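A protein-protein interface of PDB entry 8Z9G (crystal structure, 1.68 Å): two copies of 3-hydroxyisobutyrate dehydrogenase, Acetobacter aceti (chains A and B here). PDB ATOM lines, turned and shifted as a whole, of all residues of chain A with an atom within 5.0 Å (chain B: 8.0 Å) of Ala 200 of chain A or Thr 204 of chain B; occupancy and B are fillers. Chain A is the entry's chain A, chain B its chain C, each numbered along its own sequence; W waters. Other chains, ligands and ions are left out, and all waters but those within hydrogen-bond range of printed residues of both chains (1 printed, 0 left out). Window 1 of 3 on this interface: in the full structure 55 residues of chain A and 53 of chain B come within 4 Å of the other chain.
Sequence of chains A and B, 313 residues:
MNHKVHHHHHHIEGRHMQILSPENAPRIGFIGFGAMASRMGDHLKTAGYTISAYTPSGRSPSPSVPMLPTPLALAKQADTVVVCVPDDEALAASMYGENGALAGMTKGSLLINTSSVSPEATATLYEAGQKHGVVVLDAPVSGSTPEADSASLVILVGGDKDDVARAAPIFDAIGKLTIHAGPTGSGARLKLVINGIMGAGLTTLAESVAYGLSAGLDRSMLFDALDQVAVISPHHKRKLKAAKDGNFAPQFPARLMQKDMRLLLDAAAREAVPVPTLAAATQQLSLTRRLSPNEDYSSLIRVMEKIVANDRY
OG1 of Thr 277 of chain B lies within hydrogen-bond range of OG1 of Thr 203 of chain A, 2.9 Å away.
OG1 of Thr 203 of chain B sits at hydrogen-bond distance from OG1 of Thr 277 of chain A (2.9 Å).
OG1 of Thr 277 of chain A is in hydrogen-bond range of OE2 of Glu 207 of chain B, at 2.7 Å.
N of Leu 278 of chain A lies within hydrogen-bond range of OE1 of Glu 207 of chain B (3.0 Å).
The side-chain hydroxyl (OG1) of Thr 203 of chain A is in hydrogen-bond range of the backbone carbonyl oxygen (O) of Ala 200 of chain A (3.3 Å).
O of Ala 200 of chain A sits at hydrogen-bond distance from OG1 of Thr 204 of chain A (2.8 Å).
The backbone carbonyl oxygen (O) of Ala 200 of chain B lies within hydrogen-bond range of the side-chain hydroxyl (OG1) of Thr 203 of chain B (3.3 Å).
OG1 of Thr 204 of chain B is in hydrogen-bond range of O of Ala 200 of chain B, 2.8 Å away.
The backbone carbonyl oxygen of Thr 204 of chain B is in hydrogen-bond range of the side-chain hydroxyl of Ser 208 of chain B (2.9 Å).
The side-chain carboxylate (OE2) of Glu 207 of chain B is in hydrogen-bond range of the side-chain amide nitrogen (NE2) of Gln 284 of chain B (2.9 Å).
Thr 204 of chain B touches Gly 196 of chain A (CG2 to O, 3.96 Å).
Gly 196 of chain A touches Ser 208 of chain B.
Ile 197 of chain A touches Leu 205 of chain B (CD1 to CD1, 3.9 Å).
Ile 197 of chain A touches Val 231 of chain B (CG2 to O, 3.5 Å).
Ile 232 of chain B touches Ile 197 of chain A.
Val 231 of chain B touches Met 198 of chain A.
Thr 204 of chain A touches Thr 277 of chain B.
Leu 205 of chain A touches Ile 197 of chain B (CD1 to CD1, 3.8 Å).
Thr 277 of chain A touches Thr 277 of chain B.
Ser 208 of chain B touches Leu 278 of chain A (OG to CD2, 3.6 Å).
Ala 200 of chain A touches just one residue of chain B: Thr 204 (3.4 Å).
No residue of chain B comes within 4 Å of Gly 199 of chain A.
Of the printed residues of chain A, Ser 208 of chain B touches Gly 196 (3.97 Å), Ile 197 (3.5 Å) and Leu 278 (3.6 Å).
Of the printed residues of chain B, Met 198 of chain A touches Val 231.
Of the printed residues of chain A, Ile 197 of chain B touches Thr 204 (3.7 Å) and Leu 205 (3.8 Å).
Of the printed residues of chain A, Leu 205 of chain B touches Ile 197 (3.9 Å).
Of the printed residues of chain B, Gly 196 of chain A touches Thr 204 (3.96 Å) and Ser 208 (3.97 Å).
Met 261 of chain A touches none of the printed residues of chain B.
Asn 195 of chain A touches none of the printed residues of chain B.
The nearest residue of chain B that does not touch Ala 200 of chain A is Thr 277 of chain B (4.3 Å).
Of the 26 printed residues of chain B, 12 touch a printed residue of chain A.
Of the 15 printed residues of chain A, 10 touch a printed residue of chain B.
Printed residues of chain A that touch a printed residue of chain B: Gly 196, Ile 197, Met 198, Ala 200, Thr 203, Thr 204, Leu 205, Thr 277, Leu 278 and Ala 281.
Among the printed residues, 23 pairs touch across the chains.
Among the printed residues, no Asp or Glu carboxylate lies within 4 Å of a Lys or Arg side-chain nitrogen of the other chain.
Ile 197 of chain A touches Thr 204 of chain B, and with the chains exchanged Thr 204 of chain A touches Ile 197 of chain B.
Thr 204 of chain A touches Thr 277 of chain B, and with the chains exchanged Thr 277 of chain A touches Thr 204 of chain B.
Thr 277 of chain B touches its own counterpart, Thr 277 of chain A.
Thr 277 of chain A touches Ala 281 of chain B, and with the chains exchanged Ala 281 of chain A touches Thr 277 of chain B.
13 positions are printed for both chains.
Water W1 lies within hydrogen-bond range of the side-chain hydroxyl (OG1) of Thr 204 of chain B (3.3 Å), the side-chain hydroxyl (OG1) of Thr 204 of chain A (3.3 Å), the backbone carbonyl oxygen (O) of Ala 200 of chain A (3.4 Å) and the backbone carbonyl oxygen (O) of Ala 200 of chain B (3.5 Å).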
ATOM      1  N   ASN A 195      24.499  30.493   4.940  1.00  0.00           N
ATOM      2  CA  ASN A 195      24.455  29.043   4.759  1.00  0.00           C
ATOM      3  C   ASN A 195      25.077  28.321   5.946  1.00  0.00           C
ATOM      4  O   ASN A 195      24.597  27.260   6.356  1.00  0.00           O
ATOM      5  CB  ASN A 195      25.198  28.646   3.490  1.00  0.00           C
ATOM      6  CG  ASN A 195      24.376  28.835   2.244  1.00  0.00           C
ATOM      7  OD1 ASN A 195      23.138  28.798   2.275  1.00  0.00           O
ATOM      8  ND2 ASN A 195      25.059  28.988   1.125  1.00  0.00           N
ATOM      9  N   GLY A 196      26.181  28.855   6.478  1.00  0.00           N
ATOM     10  CA  GLY A 196      26.804  28.234   7.627  1.00  0.00           C
ATOM     11  C   GLY A 196      25.898  28.245   8.838  1.00  0.00           C
ATOM     12  O   GLY A 196      25.814  27.260   9.566  1.00  0.00           O
ATOM     13  N   ILE A 197      25.196  29.361   9.058  1.00  0.00           N
ATOM     14  CA  ILE A 197      24.249  29.436  10.166  1.00  0.00           C
ATOM     15  C   ILE A 197      23.125  28.417   9.978  1.00  0.00           C
ATOM     16  O   ILE A 197      22.699  27.751  10.926  1.00  0.00           O
ATOM     17  CB  ILE A 197      23.688  30.866  10.284  1.00  0.00           C
ATOM     18  CG1 ILE A 197      24.787  31.839  10.738  1.00  0.00           C
ATOM     19  CG2 ILE A 197      22.511  30.889  11.245  1.00  0.00           C
ATOM     20  CD1 ILE A 197      24.508  33.304  10.375  1.00  0.00           C
ATOM     21  N   MET A 198      22.622  28.291   8.757  1.00  0.00           N
ATOM     22  CA  MET A 198      21.550  27.323   8.518  1.00  0.00           C
ATOM     23  C   MET A 198      22.036  25.891   8.701  1.00  0.00           C
ATOM     24  O   MET A 198      21.380  25.085   9.377  1.00  0.00           O
ATOM     25  CB  MET A 198      20.963  27.529   7.121  1.00  0.00           C
ATOM     26  CG  MET A 198      19.711  26.682   6.899  1.00  0.00           C
ATOM     27  SD  MET A 198      19.175  26.977   5.212  1.00  0.00           S
ATOM     28  CE  MET A 198      20.274  25.873   4.450  1.00  0.00           C
ATOM     29  N   GLY A 199      23.178  25.551   8.100  1.00  0.00           N
ATOM     30  CA  GLY A 199      23.657  24.181   8.192  1.00  0.00           C
ATOM     31  C   GLY A 199      23.971  23.775   9.619  1.00  0.00           C
ATOM     32  O   GLY A 199      23.512  22.737  10.102  1.00  0.00           O
ATOM     33  N   ALA A 200      24.772  24.586  10.316  1.00  0.00           N
ATOM     34  CA  ALA A 200      25.127  24.234  11.688  1.00  0.00           C
ATOM     35  C   ALA A 200      23.934  24.367  12.634  1.00  0.00           C
ATOM     36  O   ALA A 200      23.895  23.709  13.677  1.00  0.00           O
ATOM     37  CB  ALA A 200      26.310  25.102  12.165  1.00  0.00           C
ATOM     38  N   GLY A 201      22.958  25.215  12.304  1.00  0.00           N
ATOM     39  CA  GLY A 201      21.747  25.254  13.111  1.00  0.00           C
ATOM     40  C   GLY A 201      21.009  23.930  13.074  1.00  0.00           C
ATOM     41  O   GLY A 201      20.485  23.463  14.092  1.00  0.00           O
ATOM     42  N   LEU A 202      20.978  23.296  11.897  1.00  0.00           N
ATOM     43  CA  LEU A 202      20.326  21.999  11.761  1.00  0.00           C
ATOM     44  C   LEU A 202      21.134  20.908  12.449  1.00  0.00           C
ATOM     45  O   LEU A 202      20.568  20.056  13.150  1.00  0.00           O
ATOM     46  CB  LEU A 202      20.131  21.678  10.274  1.00  0.00           C
ATOM     47  CG  LEU A 202      19.237  20.468   9.916  1.00  0.00           C
ATOM     48  CD1 LEU A 202      19.989  19.140  10.035  1.00  0.00           C
ATOM     49  CD2 LEU A 202      17.972  20.432  10.766  1.00  0.00           C
ATOM     50  N   THR A 203      22.463  20.897  12.259  1.00  0.00           N
ATOM     51  CA  THR A 203      23.227  19.820  12.892  1.00  0.00           C
ATOM     52  C   THR A 203      23.189  19.938  14.411  1.00  0.00           C
ATOM     53  O   THR A 203      23.098  18.919  15.116  1.00  0.00           O
ATOM     54  CB  THR A 203      24.672  19.761  12.380  1.00  0.00           C
ATOM     55  OG1 THR A 203      25.431  20.882  12.876  1.00  0.00           O
ATOM     56  CG2 THR A 203      24.713  19.766  10.863  1.00  0.00           C
ATOM     57  N   THR A 204      23.228  21.172  14.935  1.00  0.00           N
ATOM     58  CA  THR A 204      23.053  21.400  16.371  1.00  0.00           C
ATOM     59  C   THR A 204      21.740  20.815  16.866  1.00  0.00           C
ATOM     60  O   THR A 204      21.698  20.115  17.889  1.00  0.00           O
ATOM     61  CB  THR A 204      23.087  22.903  16.664  1.00  0.00           C
ATOM     62  OG1 THR A 204      24.405  23.384  16.430  1.00  0.00           O
ATOM     63  CG2 THR A 204      22.706  23.196  18.123  1.00  0.00           C
ATOM     64  N   LEU A 205      20.650  21.120  16.159  1.00  0.00           N
ATOM     65  CA  LEU A 205      19.334  20.629  16.563  1.00  0.00           C
ATOM     66  C   LEU A 205      19.249  19.108  16.489  1.00  0.00           C
ATOM     67  O   LEU A 205      18.759  18.459  17.426  1.00  0.00           O
ATOM     68  CB  LEU A 205      18.268  21.291  15.684  1.00  0.00           C
ATOM     69  CG  LEU A 205      16.817  20.911  15.950  1.00  0.00           C
ATOM     70  CD1 LEU A 205      16.421  21.227  17.399  1.00  0.00           C
ATOM     71  CD2 LEU A 205      15.931  21.657  14.939  1.00  0.00           C
ATOM     72  N   MET A 261      28.283  23.995   2.303  1.00  0.00           N
ATOM     73  CA  MET A 261      29.192  23.931   3.450  1.00  0.00           C
ATOM     74  C   MET A 261      30.628  23.720   2.988  1.00  0.00           C
ATOM     75  O   MET A 261      31.553  24.318   3.544  1.00  0.00           O
ATOM     76  CB  MET A 261      28.783  22.820   4.422  1.00  0.00           C
ATOM     77  CG  MET A 261      27.423  23.005   5.078  1.00  0.00           C
ATOM     78  SD  MET A 261      27.168  24.489   6.059  1.00  0.00           S
ATOM     79  CE  MET A 261      28.172  24.163   7.524  1.00  0.00           C
ATOM     80  N   THR A 277      32.936  24.927  14.990  1.00  0.00           N
ATOM     81  CA  THR A 277      31.529  24.512  14.978  1.00  0.00           C
ATOM     82  C   THR A 277      31.051  24.296  13.550  1.00  0.00           C
ATOM     83  O   THR A 277      30.376  23.303  13.247  1.00  0.00           O
ATOM     84  CB  THR A 277      30.639  25.547  15.675  1.00  0.00           C
ATOM     85  OG1 THR A 277      31.216  25.929  16.916  1.00  0.00           O
ATOM     86  CG2 THR A 277      29.267  24.945  15.969  1.00  0.00           C
ATOM     87  N   LEU A 278      31.393  25.230  12.653  1.00  0.00           N
ATOM     88  CA  LEU A 278      31.007  25.082  11.252  1.00  0.00           C
ATOM     89  C   LEU A 278      31.692  23.879  10.621  1.00  0.00           C
ATOM     90  O   LEU A 278      31.126  23.216   9.739  1.00  0.00           O
ATOM     91  CB  LEU A 278      31.358  26.356  10.473  1.00  0.00           C
ATOM     92  CG  LEU A 278      30.690  27.644  10.935  1.00  0.00           C
ATOM     93  CD1 LEU A 278      31.126  28.825  10.045  1.00  0.00           C
ATOM     94  CD2 LEU A 278      29.190  27.487  10.900  1.00  0.00           C
ATOM     95  N   ALA A 281      29.884  20.734  11.716  1.00  0.00           N
ATOM     96  CA  ALA A 281      28.588  20.647  11.043  1.00  0.00           C
ATOM     97  C   ALA A 281      28.737  20.149   9.617  1.00  0.00           C
ATOM     98  O   ALA A 281      27.908  19.364   9.132  1.00  0.00           O
ATOM     99  CB  ALA A 281      27.906  22.017  11.050  1.00  0.00           C
ATOM    100  N   GLY B 196      22.360  22.834  24.845  1.00  0.00           N
ATOM    101  CA  GLY B 196      23.163  22.569  23.659  1.00  0.00           C
ATOM    102  C   GLY B 196      22.763  23.441  22.491  1.00  0.00           C
ATOM    103  O   GLY B 196      23.612  23.979  21.776  1.00  0.00           O
ATOM    104  N   ILE B 197      21.451  23.565  22.266  1.00  0.00           N
ATOM    105  CA  ILE B 197      20.949  24.373  21.163  1.00  0.00           C
ATOM    106  C   ILE B 197      21.351  25.833  21.346  1.00  0.00           C
ATOM    107  O   ILE B 197      21.773  26.502  20.395  1.00  0.00           O
ATOM    108  CB  ILE B 197      19.425  24.212  21.062  1.00  0.00           C
ATOM    109  CG1 ILE B 197      19.085  22.758  20.736  1.00  0.00           C
ATOM    110  CG2 ILE B 197      18.843  25.198  20.056  1.00  0.00           C
ATOM    111  CD1 ILE B 197      17.576  22.468  20.830  1.00  0.00           C
ATOM    112  N   MET B 198      21.209  26.349  22.566  1.00  0.00           N
ATOM    113  CA  MET B 198      21.622  27.723  22.868  1.00  0.00           C
ATOM    114  C   MET B 198      23.112  27.932  22.623  1.00  0.00           C
ATOM    115  O   MET B 198      23.529  28.913  21.979  1.00  0.00           O
ATOM    116  CB  MET B 198      21.350  28.031  24.334  1.00  0.00           C
ATOM    117  CG  MET B 198      21.652  29.469  24.686  1.00  0.00           C
ATOM    118  SD  MET B 198      20.633  29.994  26.055  1.00  0.00           S
ATOM    119  CE  MET B 198      21.615  29.252  27.306  1.00  0.00           C
ATOM    120  N   GLY B 199      23.932  27.043  23.192  1.00  0.00           N
ATOM    121  CA  GLY B 199      25.376  27.240  23.162  1.00  0.00           C
ATOM    122  C   GLY B 199      25.947  27.113  21.765  1.00  0.00           C
ATOM    123  O   GLY B 199      26.710  27.968  21.313  1.00  0.00           O
ATOM    124  N   ALA B 200      25.577  26.044  21.054  1.00  0.00           N
ATOM    125  CA  ALA B 200      26.082  25.895  19.703  1.00  0.00           C
ATOM    126  C   ALA B 200      25.454  26.910  18.768  1.00  0.00           C
ATOM    127  O   ALA B 200      26.074  27.288  17.775  1.00  0.00           O
ATOM    128  CB  ALA B 200      25.842  24.462  19.204  1.00  0.00           C
ATOM    129  N   GLY B 201      24.245  27.389  19.083  1.00  0.00           N
ATOM    130  CA  GLY B 201      23.663  28.438  18.268  1.00  0.00           C
ATOM    131  C   GLY B 201      24.512  29.694  18.308  1.00  0.00           C
ATOM    132  O   GLY B 201      24.714  30.356  17.291  1.00  0.00           O
ATOM    133  N   LEU B 202      25.043  30.018  19.482  1.00  0.00           N
ATOM    134  CA  LEU B 202      25.895  31.195  19.597  1.00  0.00           C
ATOM    135  C   LEU B 202      27.247  30.969  18.932  1.00  0.00           C
ATOM    136  O   LEU B 202      27.751  31.854  18.239  1.00  0.00           O
ATOM    137  CB  LEU B 202      26.055  31.564  21.068  1.00  0.00           C
ATOM    138  CG  LEU B 202      26.712  32.916  21.408  1.00  0.00           C
ATOM    139  CD1 LEU B 202      28.242  32.863  21.316  1.00  0.00           C
ATOM    140  CD2 LEU B 202      26.151  34.045  20.545  1.00  0.00           C
ATOM    141  N   THR B 203      27.870  29.802  19.141  1.00  0.00           N
ATOM    142  CA  THR B 203      29.189  29.622  18.530  1.00  0.00           C
ATOM    143  C   THR B 203      29.095  29.586  17.014  1.00  0.00           C
ATOM    144  O   THR B 203      29.966  30.126  16.325  1.00  0.00           O
ATOM    145  CB  THR B 203      29.895  28.365  19.069  1.00  0.00           C
ATOM    146  OG1 THR B 203      29.260  27.168  18.598  1.00  0.00           O
ATOM    147  CG2 THR B 203      29.892  28.345  20.585  1.00  0.00           C
ATOM    148  N   THR B 204      28.047  28.955  16.476  1.00  0.00           N
ATOM    149  CA  THR B 204      27.779  29.001  15.041  1.00  0.00           C
ATOM    150  C   THR B 204      27.724  30.434  14.531  1.00  0.00           C
ATOM    151  O   THR B 204      28.309  30.777  13.496  1.00  0.00           O
ATOM    152  CB  THR B 204      26.447  28.309  14.764  1.00  0.00           C
ATOM    153  OG1 THR B 204      26.582  26.902  15.007  1.00  0.00           O
ATOM    154  CG2 THR B 204      25.990  28.542  13.311  1.00  0.00           C
ATOM    155  N   LEU B 205      26.985  31.275  15.237  1.00  0.00           N
ATOM    156  CA  LEU B 205      26.807  32.651  14.807  1.00  0.00           C
ATOM    157  C   LEU B 205      28.117  33.433  14.884  1.00  0.00           C
ATOM    158  O   LEU B 205      28.453  34.188  13.965  1.00  0.00           O
ATOM    159  CB  LEU B 205      25.721  33.292  15.670  1.00  0.00           C
ATOM    160  CG  LEU B 205      25.328  34.729  15.340  1.00  0.00           C
ATOM    161  CD1 LEU B 205      24.861  34.863  13.904  1.00  0.00           C
ATOM    162  CD2 LEU B 205      24.250  35.180  16.328  1.00  0.00           C
ATOM    163  N   ALA B 206      28.884  33.247  15.955  1.00  0.00           N
ATOM    164  CA  ALA B 206      30.140  33.980  16.103  1.00  0.00           C
ATOM    165  C   ALA B 206      31.129  33.596  15.007  1.00  0.00           C
ATOM    166  O   ALA B 206      31.866  34.438  14.487  1.00  0.00           O
ATOM    167  CB  ALA B 206      30.737  33.709  17.493  1.00  0.00           C
ATOM    168  N   GLU B 207      31.144  32.317  14.643  1.00  0.00           N
ATOM    169  CA  GLU B 207      32.074  31.807  13.651  1.00  0.00           C
ATOM    170  C   GLU B 207      31.674  32.288  12.264  1.00  0.00           C
ATOM    171  O   GLU B 207      32.526  32.607  11.430  1.00  0.00           O
ATOM    172  CB  GLU B 207      31.992  30.297  13.768  1.00  0.00           C
ATOM    173  CG  GLU B 207      32.833  29.790  14.911  1.00  0.00           C
ATOM    174  CD  GLU B 207      32.870  28.300  14.992  1.00  0.00           C
ATOM    175  OE1 GLU B 207      32.622  27.654  13.968  1.00  0.00           O
ATOM    176  OE2 GLU B 207      33.037  27.790  16.136  1.00  0.00           O
ATOM    177  N   SER B 208      30.362  32.295  11.993  1.00  0.00           N
ATOM    178  CA  SER B 208      29.869  32.722  10.690  1.00  0.00           C
ATOM    179  C   SER B 208      30.095  34.209  10.502  1.00  0.00           C
ATOM    180  O   SER B 208      30.526  34.640   9.430  1.00  0.00           O
ATOM    181  CB  SER B 208      28.387  32.375  10.531  1.00  0.00           C
ATOM    182  OG  SER B 208      28.192  30.974  10.578  1.00  0.00           O
ATOM    183  N   VAL B 209      29.846  34.993  11.554  1.00  0.00           N
ATOM    184  CA  VAL B 209      30.167  36.419  11.519  1.00  0.00           C
ATOM    185  C   VAL B 209      31.659  36.623  11.291  1.00  0.00           C
ATOM    186  O   VAL B 209      32.068  37.473  10.490  1.00  0.00           O
ATOM    187  CB  VAL B 209      29.691  37.095  12.816  1.00  0.00           C
ATOM    188  CG1 VAL B 209      30.323  38.499  12.974  1.00  0.00           C
ATOM    189  CG2 VAL B 209      28.179  37.183  12.846  1.00  0.00           C
ATOM    190  N   ALA B 210      32.496  35.841  11.981  1.00  0.00           N
ATOM    191  CA  ALA B 210      33.940  36.004  11.821  1.00  0.00           C
ATOM    192  C   ALA B 210      34.371  35.734  10.387  1.00  0.00           C
ATOM    193  O   ALA B 210      35.192  36.476   9.840  1.00  0.00           O
ATOM    194  CB  ALA B 210      34.688  35.090  12.802  1.00  0.00           C
ATOM    195  N   TYR B 211      33.847  34.672   9.755  1.00  0.00           N
ATOM    196  CA  TYR B 211      34.170  34.465   8.347  1.00  0.00           C
ATOM    197  C   TYR B 211      33.773  35.694   7.536  1.00  0.00           C
ATOM    198  O   TYR B 211      34.551  36.195   6.712  1.00  0.00           O
ATOM    199  CB  TYR B 211      33.490  33.204   7.756  1.00  0.00           C
ATOM    200  CG  TYR B 211      33.575  33.307   6.257  1.00  0.00           C
ATOM    201  CD1 TYR B 211      34.811  33.202   5.606  1.00  0.00           C
ATOM    202  CD2 TYR B 211      32.456  33.641   5.486  1.00  0.00           C
ATOM    203  CE1 TYR B 211      34.923  33.397   4.224  1.00  0.00           C
ATOM    204  CE2 TYR B 211      32.568  33.840   4.121  1.00  0.00           C
ATOM    205  CZ  TYR B 211      33.797  33.710   3.499  1.00  0.00           C
ATOM    206  OH  TYR B 211      33.899  33.922   2.141  1.00  0.00           O
ATOM    207  N   LEU B 226      21.947  40.008   9.089  1.00  0.00           N
ATOM    208  CA  LEU B 226      21.616  38.803   9.840  1.00  0.00           C
ATOM    209  C   LEU B 226      20.396  39.005  10.732  1.00  0.00           C
ATOM    210  O   LEU B 226      19.684  38.043  11.034  1.00  0.00           O
ATOM    211  CB  LEU B 226      22.830  38.361  10.667  1.00  0.00           C
ATOM    212  CG  LEU B 226      24.012  37.907   9.808  1.00  0.00           C
ATOM    213  CD1 LEU B 226      25.155  37.376  10.666  1.00  0.00           C
ATOM    214  CD2 LEU B 226      23.577  36.854   8.780  1.00  0.00           C
ATOM    215  N   VAL B 231      16.929  32.170   9.778  1.00  0.00           N
ATOM    216  CA  VAL B 231      17.682  31.013  10.251  1.00  0.00           C
ATOM    217  C   VAL B 231      18.397  31.291  11.577  1.00  0.00           C
ATOM    218  O   VAL B 231      19.153  30.444  12.050  1.00  0.00           O
ATOM    219  CB  VAL B 231      18.675  30.513   9.181  1.00  0.00           C
ATOM    220  CG1 VAL B 231      17.923  29.939   7.974  1.00  0.00           C
ATOM    221  CG2 VAL B 231      19.643  31.628   8.738  1.00  0.00           C
ATOM    222  N   ILE B 232      18.155  32.450  12.196  1.00  0.00           N
ATOM    223  CA  ILE B 232      18.666  32.777  13.531  1.00  0.00           C
ATOM    224  C   ILE B 232      17.486  32.894  14.485  1.00  0.00           C
ATOM    225  O   ILE B 232      16.453  33.477  14.137  1.00  0.00           O
ATOM    226  CB  ILE B 232      19.492  34.078  13.527  1.00  0.00           C
ATOM    227  CG1 ILE B 232      20.656  33.979  12.535  1.00  0.00           C
ATOM    228  CG2 ILE B 232      20.028  34.370  14.930  1.00  0.00           C
ATOM    229  CD1 ILE B 232      21.357  35.311  12.305  1.00  0.00           C
ATOM    230  N   HIS B 236      19.086  34.441  19.841  1.00  0.00           N
ATOM    231  CA  HIS B 236      20.401  34.750  19.292  1.00  0.00           C
ATOM    232  C   HIS B 236      20.398  36.064  18.522  1.00  0.00           C
ATOM    233  O   HIS B 236      21.443  36.724  18.442  1.00  0.00           O
ATOM    234  CB  HIS B 236      20.886  33.574  18.432  1.00  0.00           C
ATOM    235  CG  HIS B 236      21.172  32.343  19.242  1.00  0.00           C
ATOM    236  ND1 HIS B 236      20.334  31.247  19.263  1.00  0.00           N
ATOM    237  CD2 HIS B 236      22.192  32.051  20.086  1.00  0.00           C
ATOM    238  CE1 HIS B 236      20.829  30.330  20.077  1.00  0.00           C
ATOM    239  NE2 HIS B 236      21.956  30.796  20.592  1.00  0.00           N
ATOM    240  N   THR B 277      29.018  18.662  16.549  1.00  0.00           N
ATOM    241  CA  THR B 277      28.756  20.107  16.539  1.00  0.00           C
ATOM    242  C   THR B 277      28.704  20.654  17.963  1.00  0.00           C
ATOM    243  O   THR B 277      29.275  21.712  18.254  1.00  0.00           O
ATOM    244  CB  THR B 277      27.455  20.423  15.784  1.00  0.00           C
ATOM    245  OG1 THR B 277      27.423  19.674  14.558  1.00  0.00           O
ATOM    246  CG2 THR B 277      27.395  21.915  15.449  1.00  0.00           C
ATOM    247  N   LEU B 278      28.041  19.930  18.871  1.00  0.00           N
ATOM    248  CA  LEU B 278      27.982  20.347  20.267  1.00  0.00           C
ATOM    249  C   LEU B 278      29.359  20.299  20.912  1.00  0.00           C
ATOM    250  O   LEU B 278      29.685  21.146  21.752  1.00  0.00           O
ATOM    251  CB  LEU B 278      27.012  19.441  21.046  1.00  0.00           C
ATOM    252  CG  LEU B 278      25.581  19.426  20.503  1.00  0.00           C
ATOM    253  CD1 LEU B 278      24.714  18.522  21.333  1.00  0.00           C
ATOM    254  CD2 LEU B 278      24.996  20.824  20.530  1.00  0.00           C
ATOM    255  N   ALA B 281      31.355  23.318  19.792  1.00  0.00           N
ATOM    256  CA  ALA B 281      30.821  24.503  20.450  1.00  0.00           C
ATOM    257  C   ALA B 281      31.343  24.615  21.868  1.00  0.00           C
ATOM    258  O   ALA B 281      31.706  25.708  22.320  1.00  0.00           O
ATOM    259  CB  ALA B 281      29.294  24.457  20.477  1.00  0.00           C
ATOM    260  N   GLN B 284      34.786  26.111  21.998  1.00  0.00           N
ATOM    261  CA  GLN B 284      34.754  27.554  21.787  1.00  0.00           C
ATOM    262  C   GLN B 284      34.266  28.279  23.034  1.00  0.00           C
ATOM    263  O   GLN B 284      34.730  29.384  23.347  1.00  0.00           O
ATOM    264  CB  GLN B 284      33.848  27.872  20.598  1.00  0.00           C
ATOM    265  CG  GLN B 284      34.411  27.444  19.260  1.00  0.00           C
ATOM    266  CD  GLN B 284      35.389  28.456  18.717  1.00  0.00           C
ATOM    267  OE1 GLN B 284      36.513  28.576  19.210  1.00  0.00           O
ATOM    268  NE2 GLN B 284      34.970  29.202  17.701  1.00  0.00           N
ATOM    269  N   LEU B 300      31.847  35.540  22.978  1.00  0.00           N
ATOM    270  CA  LEU B 300      32.581  34.845  21.921  1.00  0.00           C
ATOM    271  C   LEU B 300      32.500  35.597  20.600  1.00  0.00           C
ATOM    272  O   LEU B 300      33.419  35.511  19.778  1.00  0.00           O
ATOM    273  CB  LEU B 300      32.041  33.413  21.763  1.00  0.00           C
ATOM    274  CG  LEU B 300      32.675  32.585  20.645  1.00  0.00           C
ATOM    275  CD1 LEU B 300      34.161  32.378  20.935  1.00  0.00           C
ATOM    276  CD2 LEU B 300      31.943  31.222  20.526  1.00  0.00           C
ATOM    277  N   ILE B 301      31.408  36.330  20.355  1.00  0.00           N
ATOM    278  CA  ILE B 301      31.346  37.110  19.123  1.00  0.00           C
ATOM    279  C   ILE B 301      32.490  38.114  19.082  1.00  0.00           C
ATOM    280  O   ILE B 301      33.181  38.243  18.067  1.00  0.00           O
ATOM    281  CB  ILE B 301      29.976  37.797  18.966  1.00  0.00           C
ATOM    282  CG1 ILE B 301      28.895  36.735  18.736  1.00  0.00           C
ATOM    283  CG2 ILE B 301      29.983  38.717  17.762  1.00  0.00           C
ATOM    284  CD1 ILE B 301      27.482  37.232  18.951  1.00  0.00           C
HETATM  285  O   HOH W   1      23.424  26.434  15.678  1.00  0.00           O
